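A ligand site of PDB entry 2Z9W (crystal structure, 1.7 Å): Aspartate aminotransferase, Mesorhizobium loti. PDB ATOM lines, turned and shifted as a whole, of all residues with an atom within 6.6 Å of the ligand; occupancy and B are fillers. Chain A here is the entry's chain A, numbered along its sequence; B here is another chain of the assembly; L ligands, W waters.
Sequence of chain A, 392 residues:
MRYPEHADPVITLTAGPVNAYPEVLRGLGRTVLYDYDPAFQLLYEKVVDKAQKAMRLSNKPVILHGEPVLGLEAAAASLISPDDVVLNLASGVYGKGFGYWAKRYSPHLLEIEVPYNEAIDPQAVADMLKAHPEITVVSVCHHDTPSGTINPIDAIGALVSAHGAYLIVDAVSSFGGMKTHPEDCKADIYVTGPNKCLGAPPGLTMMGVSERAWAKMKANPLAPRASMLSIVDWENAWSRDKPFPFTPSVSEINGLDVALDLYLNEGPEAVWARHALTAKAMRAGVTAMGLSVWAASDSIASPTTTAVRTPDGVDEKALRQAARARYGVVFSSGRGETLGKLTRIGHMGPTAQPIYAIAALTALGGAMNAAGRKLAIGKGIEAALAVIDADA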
ATOM      1  N   ALA A  15      -9.438  16.360  29.967  1.00  0.00           N
ATOM      2  CA  ALA A  15     -10.663  15.576  29.705  1.00  0.00           C
ATOM      3  C   ALA A  15     -10.826  15.211  28.235  1.00  0.00           C
ATOM      4  O   ALA A  15     -11.933  14.885  27.787  1.00  0.00           O
ATOM      5  CB  ALA A  15     -11.901  16.345  30.206  1.00  0.00           C
ATOM      6  N   GLY A  16      -9.723  15.241  27.479  1.00  0.00           N
ATOM      7  CA  GLY A  16      -9.748  14.811  26.086  1.00  0.00           C
ATOM      8  C   GLY A  16      -9.146  15.824  25.130  1.00  0.00           C
ATOM      9  O   GLY A  16      -9.534  17.000  25.134  1.00  0.00           O
ATOM     10  N   GLU A  67     -12.571  10.118  14.377  1.00  0.00           N
ATOM     11  CA  GLU A  67     -12.885  10.255  15.803  1.00  0.00           C
ATOM     12  C   GLU A  67     -14.404  10.451  15.968  1.00  0.00           C
ATOM     13  O   GLU A  67     -15.120  10.714  14.989  1.00  0.00           O
ATOM     14  CB  GLU A  67     -11.965  11.269  16.500  1.00  0.00           C
ATOM     15  CG  GLU A  67     -12.349  12.702  16.494  1.00  0.00           C
ATOM     16  CD  GLU A  67     -13.174  13.082  17.732  1.00  0.00           C
ATOM     17  OE1 GLU A  67     -14.276  13.568  17.516  1.00  0.00           O
ATOM     18  OE2 GLU A  67     -12.717  12.904  18.885  1.00  0.00           O
ATOM     19  N   PRO A  68     -14.927  10.209  17.173  1.00  0.00           N
ATOM     20  CA  PRO A  68     -16.377  10.084  17.372  1.00  0.00           C
ATOM     21  C   PRO A  68     -17.330  11.171  16.882  1.00  0.00           C
ATOM     22  O   PRO A  68     -18.515  10.856  16.692  1.00  0.00           O
ATOM     23  CB  PRO A  68     -16.486   9.851  18.899  1.00  0.00           C
ATOM     24  CG  PRO A  68     -15.229   9.084  19.178  1.00  0.00           C
ATOM     25  CD  PRO A  68     -14.196   9.869  18.404  1.00  0.00           C
ATOM     26  N   VAL A  69     -16.878  12.405  16.640  1.00  0.00           N
ATOM     27  CA  VAL A  69     -17.776  13.373  15.972  1.00  0.00           C
ATOM     28  C   VAL A  69     -18.270  12.816  14.626  1.00  0.00           C
ATOM     29  O   VAL A  69     -19.384  13.130  14.201  1.00  0.00           O
ATOM     30  CB  VAL A  69     -17.190  14.784  15.760  1.00  0.00           C
ATOM     31  CG1 VAL A  69     -16.982  15.487  17.095  1.00  0.00           C
ATOM     32  CG2 VAL A  69     -15.901  14.745  14.948  1.00  0.00           C
ATOM     33  N   LEU A  72     -21.298  10.687  15.507  1.00  0.00           N
ATOM     34  CA  LEU A  72     -22.450  11.548  15.842  1.00  0.00           C
ATOM     35  C   LEU A  72     -23.097  12.129  14.583  1.00  0.00           C
ATOM     36  O   LEU A  72     -24.303  12.041  14.381  1.00  0.00           O
ATOM     37  CB  LEU A  72     -22.057  12.662  16.820  1.00  0.00           C
ATOM     38  CG  LEU A  72     -21.494  12.198  18.167  1.00  0.00           C
ATOM     39  CD1 LEU A  72     -20.967  13.418  18.956  1.00  0.00           C
ATOM     40  CD2 LEU A  72     -22.557  11.426  18.974  1.00  0.00           C
ATOM     41  N   TYR A  94     -22.238  19.578  24.050  1.00  0.00           N
ATOM     42  CA  TYR A  94     -22.426  18.483  23.083  1.00  0.00           C
ATOM     43  C   TYR A  94     -23.907  18.246  22.813  1.00  0.00           C
ATOM     44  O   TYR A  94     -24.315  18.107  21.666  1.00  0.00           O
ATOM     45  CB  TYR A  94     -21.742  17.200  23.561  1.00  0.00           C
ATOM     46  CG  TYR A  94     -20.255  17.193  23.298  1.00  0.00           C
ATOM     47  CD1 TYR A  94     -19.762  16.846  22.043  1.00  0.00           C
ATOM     48  CD2 TYR A  94     -19.346  17.553  24.296  1.00  0.00           C
ATOM     49  CE1 TYR A  94     -18.397  16.832  21.786  1.00  0.00           C
ATOM     50  CE2 TYR A  94     -17.978  17.557  24.047  1.00  0.00           C
ATOM     51  CZ  TYR A  94     -17.515  17.195  22.789  1.00  0.00           C
ATOM     52  OH  TYR A  94     -16.151  17.196  22.523  1.00  0.00           O
ATOM     53  N   CYS A 141     -26.981  13.139  25.300  1.00  0.00           N
ATOM     54  CA  CYS A 141     -25.581  12.963  25.614  1.00  0.00           C
ATOM     55  C   CYS A 141     -25.489  12.431  27.051  1.00  0.00           C
ATOM     56  O   CYS A 141     -26.151  12.950  27.961  1.00  0.00           O
ATOM     57  CB  CYS A 141     -24.877  14.308  25.489  1.00  0.00           C
ATOM     58  SG  CYS A 141     -23.095  14.299  25.818  1.00  0.00           S
ATOM     59  N   HIS A 142     -24.706  11.386  27.246  1.00  0.00           N
ATOM     60  CA  HIS A 142     -24.551  10.790  28.582  1.00  0.00           C
ATOM     61  C   HIS A 142     -23.739  11.648  29.552  1.00  0.00           C
ATOM     62  O   HIS A 142     -24.223  12.076  30.616  1.00  0.00           O
ATOM     63  CB  HIS A 142     -23.925   9.422  28.459  1.00  0.00           C
ATOM     64  CG  HIS A 142     -23.985   8.617  29.715  1.00  0.00           C
ATOM     65  ND1 HIS A 142     -23.264   7.457  29.891  1.00  0.00           N
ATOM     66  CD2 HIS A 142     -24.730   8.779  30.844  1.00  0.00           C
ATOM     67  CE1 HIS A 142     -23.536   6.952  31.084  1.00  0.00           C
ATOM     68  NE2 HIS A 142     -24.421   7.730  31.673  1.00  0.00           N
ATOM     69  N   HIS A 143     -22.483  11.901  29.172  1.00  0.00           N
ATOM     70  CA  HIS A 143     -21.593  12.778  29.920  1.00  0.00           C
ATOM     71  C   HIS A 143     -21.311  13.975  29.029  1.00  0.00           C
ATOM     72  O   HIS A 143     -20.582  13.851  28.045  1.00  0.00           O
ATOM     73  CB  HIS A 143     -20.309  12.009  30.273  1.00  0.00           C
ATOM     74  CG  HIS A 143     -19.219  12.826  30.912  1.00  0.00           C
ATOM     75  ND1 HIS A 143     -19.436  14.029  31.561  1.00  0.00           N
ATOM     76  CD2 HIS A 143     -17.895  12.572  31.022  1.00  0.00           C
ATOM     77  CE1 HIS A 143     -18.291  14.474  32.049  1.00  0.00           C
ATOM     78  NE2 HIS A 143     -17.338  13.615  31.727  1.00  0.00           N
ATOM     79  N   ASP A 144     -21.930  15.110  29.336  1.00  0.00           N
ATOM     80  CA  ASP A 144     -21.685  16.298  28.531  1.00  0.00           C
ATOM     81  C   ASP A 144     -20.414  16.951  29.080  1.00  0.00           C
ATOM     82  O   ASP A 144     -20.449  17.787  29.984  1.00  0.00           O
ATOM     83  CB  ASP A 144     -22.885  17.256  28.502  1.00  0.00           C
ATOM     84  CG  ASP A 144     -22.903  18.099  27.235  1.00  0.00           C
ATOM     85  OD1 ASP A 144     -21.829  18.638  26.892  1.00  0.00           O
ATOM     86  OD2 ASP A 144     -23.976  18.218  26.585  1.00  0.00           O
ATOM     87  N   THR A 145     -19.290  16.509  28.523  1.00  0.00           N
ATOM     88  CA  THR A 145     -17.978  16.687  29.141  1.00  0.00           C
ATOM     89  C   THR A 145     -17.598  18.120  29.562  1.00  0.00           C
ATOM     90  O   THR A 145     -17.019  18.309  30.637  1.00  0.00           O
ATOM     91  CB  THR A 145     -16.890  16.016  28.260  1.00  0.00           C
ATOM     92  OG1 THR A 145     -17.482  14.880  27.604  1.00  0.00           O
ATOM     93  CG2 THR A 145     -15.705  15.560  29.119  1.00  0.00           C
ATOM     94  N   PRO A 146     -17.960  19.104  28.749  1.00  0.00           N
ATOM     95  CA  PRO A 146     -17.616  20.480  29.110  1.00  0.00           C
ATOM     96  C   PRO A 146     -18.281  21.011  30.378  1.00  0.00           C
ATOM     97  O   PRO A 146     -17.968  22.069  30.826  1.00  0.00           O
ATOM     98  CB  PRO A 146     -18.040  21.277  27.885  1.00  0.00           C
ATOM     99  CG  PRO A 146     -17.896  20.349  26.776  1.00  0.00           C
ATOM    100  CD  PRO A 146     -18.291  18.984  27.326  1.00  0.00           C
ATOM    101  N   ASP A 170     -24.842   9.770  22.772  1.00  0.00           N
ATOM    102  CA  ASP A 170     -23.410  10.108  22.797  1.00  0.00           C
ATOM    103  C   ASP A 170     -22.868   9.619  24.159  1.00  0.00           C
ATOM    104  O   ASP A 170     -23.151  10.228  25.191  1.00  0.00           O
ATOM    105  CB  ASP A 170     -23.250  11.626  22.660  1.00  0.00           C
ATOM    106  CG  ASP A 170     -21.805  12.098  22.830  1.00  0.00           C
ATOM    107  OD1 ASP A 170     -21.549  13.285  22.508  1.00  0.00           O
ATOM    108  OD2 ASP A 170     -20.949  11.310  23.296  1.00  0.00           O
ATOM    109  N   ALA A 171     -22.134   8.510  24.137  1.00  0.00           N
ATOM    110  CA  ALA A 171     -21.445   8.018  25.353  1.00  0.00           C
ATOM    111  C   ALA A 171     -19.920   8.062  25.163  1.00  0.00           C
ATOM    112  O   ALA A 171     -19.180   7.221  25.691  1.00  0.00           O
ATOM    113  CB  ALA A 171     -21.902   6.630  25.674  1.00  0.00           C
ATOM    114  N   VAL A 172     -19.442   9.058  24.419  1.00  0.00           N
ATOM    115  CA  VAL A 172     -18.015   9.091  24.082  1.00  0.00           C
ATOM    116  C   VAL A 172     -17.127   9.243  25.341  1.00  0.00           C
ATOM    117  O   VAL A 172     -16.061   8.624  25.446  1.00  0.00           O
ATOM    118  CB  VAL A 172     -17.719  10.211  23.060  1.00  0.00           C
ATOM    119  CG1 VAL A 172     -16.199  10.311  22.817  1.00  0.00           C
ATOM    120  CG2 VAL A 172     -18.437   9.934  21.753  1.00  0.00           C
ATOM    121  N   SER A 173     -17.593  10.023  26.318  1.00  0.00           N
ATOM    122  CA  SER A 173     -16.774  10.323  27.489  1.00  0.00           C
ATOM    123  C   SER A 173     -17.251   9.598  28.752  1.00  0.00           C
ATOM    124  O   SER A 173     -16.835   9.953  29.855  1.00  0.00           O
ATOM    125  CB  SER A 173     -16.737  11.831  27.724  1.00  0.00           C
ATOM    126  OG  SER A 173     -18.059  12.288  27.956  1.00  0.00           O
ATOM    127  N   ASN A 195     -10.979   7.205  22.890  1.00  0.00           N
ATOM    128  CA  ASN A 195     -10.146   8.399  23.124  1.00  0.00           C
ATOM    129  C   ASN A 195     -10.448   9.188  24.380  1.00  0.00           C
ATOM    130  O   ASN A 195      -9.961  10.331  24.546  1.00  0.00           O
ATOM    131  CB  ASN A 195     -10.221   9.329  21.904  1.00  0.00           C
ATOM    132  CG  ASN A 195     -11.652   9.622  21.483  1.00  0.00           C
ATOM    133  OD1 ASN A 195     -12.429   8.712  21.157  1.00  0.00           O
ATOM    134  ND2 ASN A 195     -12.003  10.904  21.482  1.00  0.00           N
ATOM    135  N   LYS A 196     -11.305   8.649  25.240  1.00  0.00           N
ATOM    136  CA  LYS A 196     -11.521   9.217  26.549  1.00  0.00           C
ATOM    137  C   LYS A 196     -11.144   8.174  27.646  1.00  0.00           C
ATOM    138  O   LYS A 196     -10.025   7.972  27.885  1.00  0.00           O
ATOM    139  CB  LYS A 196     -12.973   9.731  26.668  1.00  0.00           C
ATOM    140  CG  LYS A 196     -13.327  10.798  25.610  1.00  0.00           C
ATOM    141  CD  LYS A 196     -12.667  12.119  25.785  1.00  0.00           C
ATOM    142  CE  LYS A 196     -12.916  13.190  24.707  1.00  0.00           C
ATOM    143  NZ  LYS A 196     -14.298  13.364  24.288  1.00  0.00           N
ATOM    144  N   ARG A 335     -15.734  24.724  27.430  1.00  0.00           N
ATOM    145  CA  ARG A 335     -15.962  24.823  25.974  1.00  0.00           C
ATOM    146  C   ARG A 335     -17.248  25.606  25.769  1.00  0.00           C
ATOM    147  O   ARG A 335     -18.179  25.492  26.557  1.00  0.00           O
ATOM    148  CB  ARG A 335     -16.057  23.427  25.344  1.00  0.00           C
ATOM    149  CG  ARG A 335     -16.210  23.437  23.814  1.00  0.00           C
ATOM    150  CD  ARG A 335     -16.238  22.031  23.210  1.00  0.00           C
ATOM    151  NE  ARG A 335     -16.690  22.060  21.815  1.00  0.00           N
ATOM    152  CZ  ARG A 335     -16.558  21.046  20.959  1.00  0.00           C
ATOM    153  NH1 ARG A 335     -15.995  19.898  21.342  1.00  0.00           N
ATOM    154  NH2 ARG A 335     -17.000  21.175  19.710  1.00  0.00           N
ATOM    155  N   ARG A 344     -11.592  21.910  34.072  1.00  0.00           N
ATOM    156  CA  ARG A 344     -11.894  20.468  34.106  1.00  0.00           C
ATOM    157  C   ARG A 344     -10.661  19.634  34.398  1.00  0.00           C
ATOM    158  O   ARG A 344      -9.607  19.815  33.795  1.00  0.00           O
ATOM    159  CB  ARG A 344     -12.523  20.022  32.804  1.00  0.00           C
ATOM    160  CG  ARG A 344     -13.935  20.517  32.620  1.00  0.00           C
ATOM    161  CD  ARG A 344     -14.511  19.965  31.341  1.00  0.00           C
ATOM    162  NE  ARG A 344     -13.887  20.549  30.151  1.00  0.00           N
ATOM    163  CZ  ARG A 344     -13.946  20.048  28.933  1.00  0.00           C
ATOM    164  NH1 ARG A 344     -14.604  18.912  28.685  1.00  0.00           N
ATOM    165  NH2 ARG A 344     -13.330  20.687  27.925  1.00  0.00           N
ATOM    166  N   MET A 348      -9.585   9.675  33.513  1.00  0.00           N
ATOM    167  CA  MET A 348      -9.871   8.858  32.318  1.00  0.00           C
ATOM    168  C   MET A 348      -8.741   7.909  32.017  1.00  0.00           C
ATOM    169  O   MET A 348      -7.606   8.342  31.821  1.00  0.00           O
ATOM    170  CB  MET A 348     -10.092   9.768  31.093  1.00  0.00           C
ATOM    171  CG  MET A 348     -11.403  10.524  31.137  1.00  0.00           C
ATOM    172  SD  MET A 348     -11.539  11.705  29.788  1.00  0.00           S
ATOM    173  CE  MET A 348     -13.289  12.108  29.937  1.00  0.00           C
ATOM    174  N   THR B 247     -11.406  17.101  17.459  1.00  0.00           N
ATOM    175  CA  THR B 247     -10.134  16.660  18.023  1.00  0.00           C
ATOM    176  C   THR B 247      -9.227  16.044  16.949  1.00  0.00           C
ATOM    177  O   THR B 247      -9.633  15.126  16.233  1.00  0.00           O
ATOM    178  CB  THR B 247     -10.368  15.683  19.179  1.00  0.00           C
ATOM    179  OG1 THR B 247     -11.207  16.315  20.142  1.00  0.00           O
ATOM    180  CG2 THR B 247      -9.053  15.344  19.822  1.00  0.00           C
HETATM  181  O1  LIG L   1     -14.925  12.512  20.529  1.00  0.00           O
HETATM  182  C1  LIG L   1     -15.882  13.552  20.457  1.00  0.00           C
HETATM  183  C2  LIG L   1     -16.732  13.675  21.739  1.00  0.00           C
HETATM  184  C3  LIG L   1     -18.114  13.584  21.607  1.00  0.00           C
HETATM  185  N1  LIG L   1     -18.902  13.693  22.671  1.00  0.00           N
HETATM  186  C4  LIG L   1     -18.422  13.927  23.906  1.00  0.00           C
HETATM  187  C5  LIG L   1     -17.044  14.015  24.099  1.00  0.00           C
HETATM  188  C6  LIG L   1     -16.184  13.899  22.999  1.00  0.00           C
HETATM  189  C7  LIG L   1     -14.688  14.005  23.161  1.00  0.00           C
HETATM  190  O2  LIG L   1     -16.541  14.253  25.340  1.00  0.00           O
HETATM  191  C8  LIG L   1     -19.402  14.035  25.066  1.00  0.00           C
HETATM  192  O   HOH W   1     -13.995  15.817  26.349  1.00  0.00           O
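Water W1 lies within hydrogen-bond range of O of Ala 15 (2.7 Å), O2 of the ligand (3.2 Å) and NZ of Lys 196 (3.2 Å).
CD of Pro 68 touches O1 of the ligand, at 3.5 Å. Leu 72 touches the ligand (CD1 to C3, 3.9 Å). Tyr 94 touches the ligand (CE1 to C3, 3.3 Å). SG of Cys 141 touches C8 of the ligand, at 3.8 Å. His 143 touches the ligand (O to C8, 3.2 Å). CG1 of Val 172 touches O1 of the ligand, 3.4 Å away. Ser 173 touches the ligand. 12 residues have an atom within 4 Å of the ligand: Glu 67, Pro 68, Leu 72, Tyr 94, Cys 141, His 143, Thr 145, Asp 170, Val 172, Ser 173, Asn 195 and Lys 196.
O of Thr 145 sits close to NH1 of Arg 344 (3.2 Å). The backbone NH (N) of Val 172 lies within hydrogen-bond range of the side-chain carboxylate (OD2) of Asp 170. The side-chain carboxylate (OD1) of Asp 170 lies within hydrogen-bond range of the side-chain sulfur (SG) of Cys 141 (3.8 Å). N of His 142 lies within hydrogen-bond range of O of Asp 170, at 2.8 Å. The side-chain carboxylate of Glu 67 is in hydrogen-bond range of the side-chain amide nitrogen of Asn 195, at 3.4 Å. The backbone carbonyl oxygen (O) of His 143 lies within hydrogen-bond range of the side-chain hydroxyl (OG) of Ser 173, at 3.0 Å. SG of Cys 141 sits at hydrogen-bond distance from O of His 143, at 3.4 Å. The side-chain hydroxyl (OH) of Tyr 94 lies within hydrogen-bond range of the guanidinium group (NH1) of Arg 335 (3.0 Å).
The side-chain amino group of Lys 196 is bonded to a carbon (C7) of the ligand, 1.4 Å away. O2 of the ligand sits at hydrogen-bond distance from OG1 of Thr 145, 2.5 Å away. The side-chain carboxylate of Asp 170 lies within hydrogen-bond range of a nitrogen (N1) of the ligand. The side-chain carboxylate (OE2) of Glu 67 is in hydrogen-bond range of an oxygen (O1) of the ligand, 2.8 Å away. ND2 of Asn 195 is in hydrogen-bond range of O1 of the ligand, at 3.5 Å.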
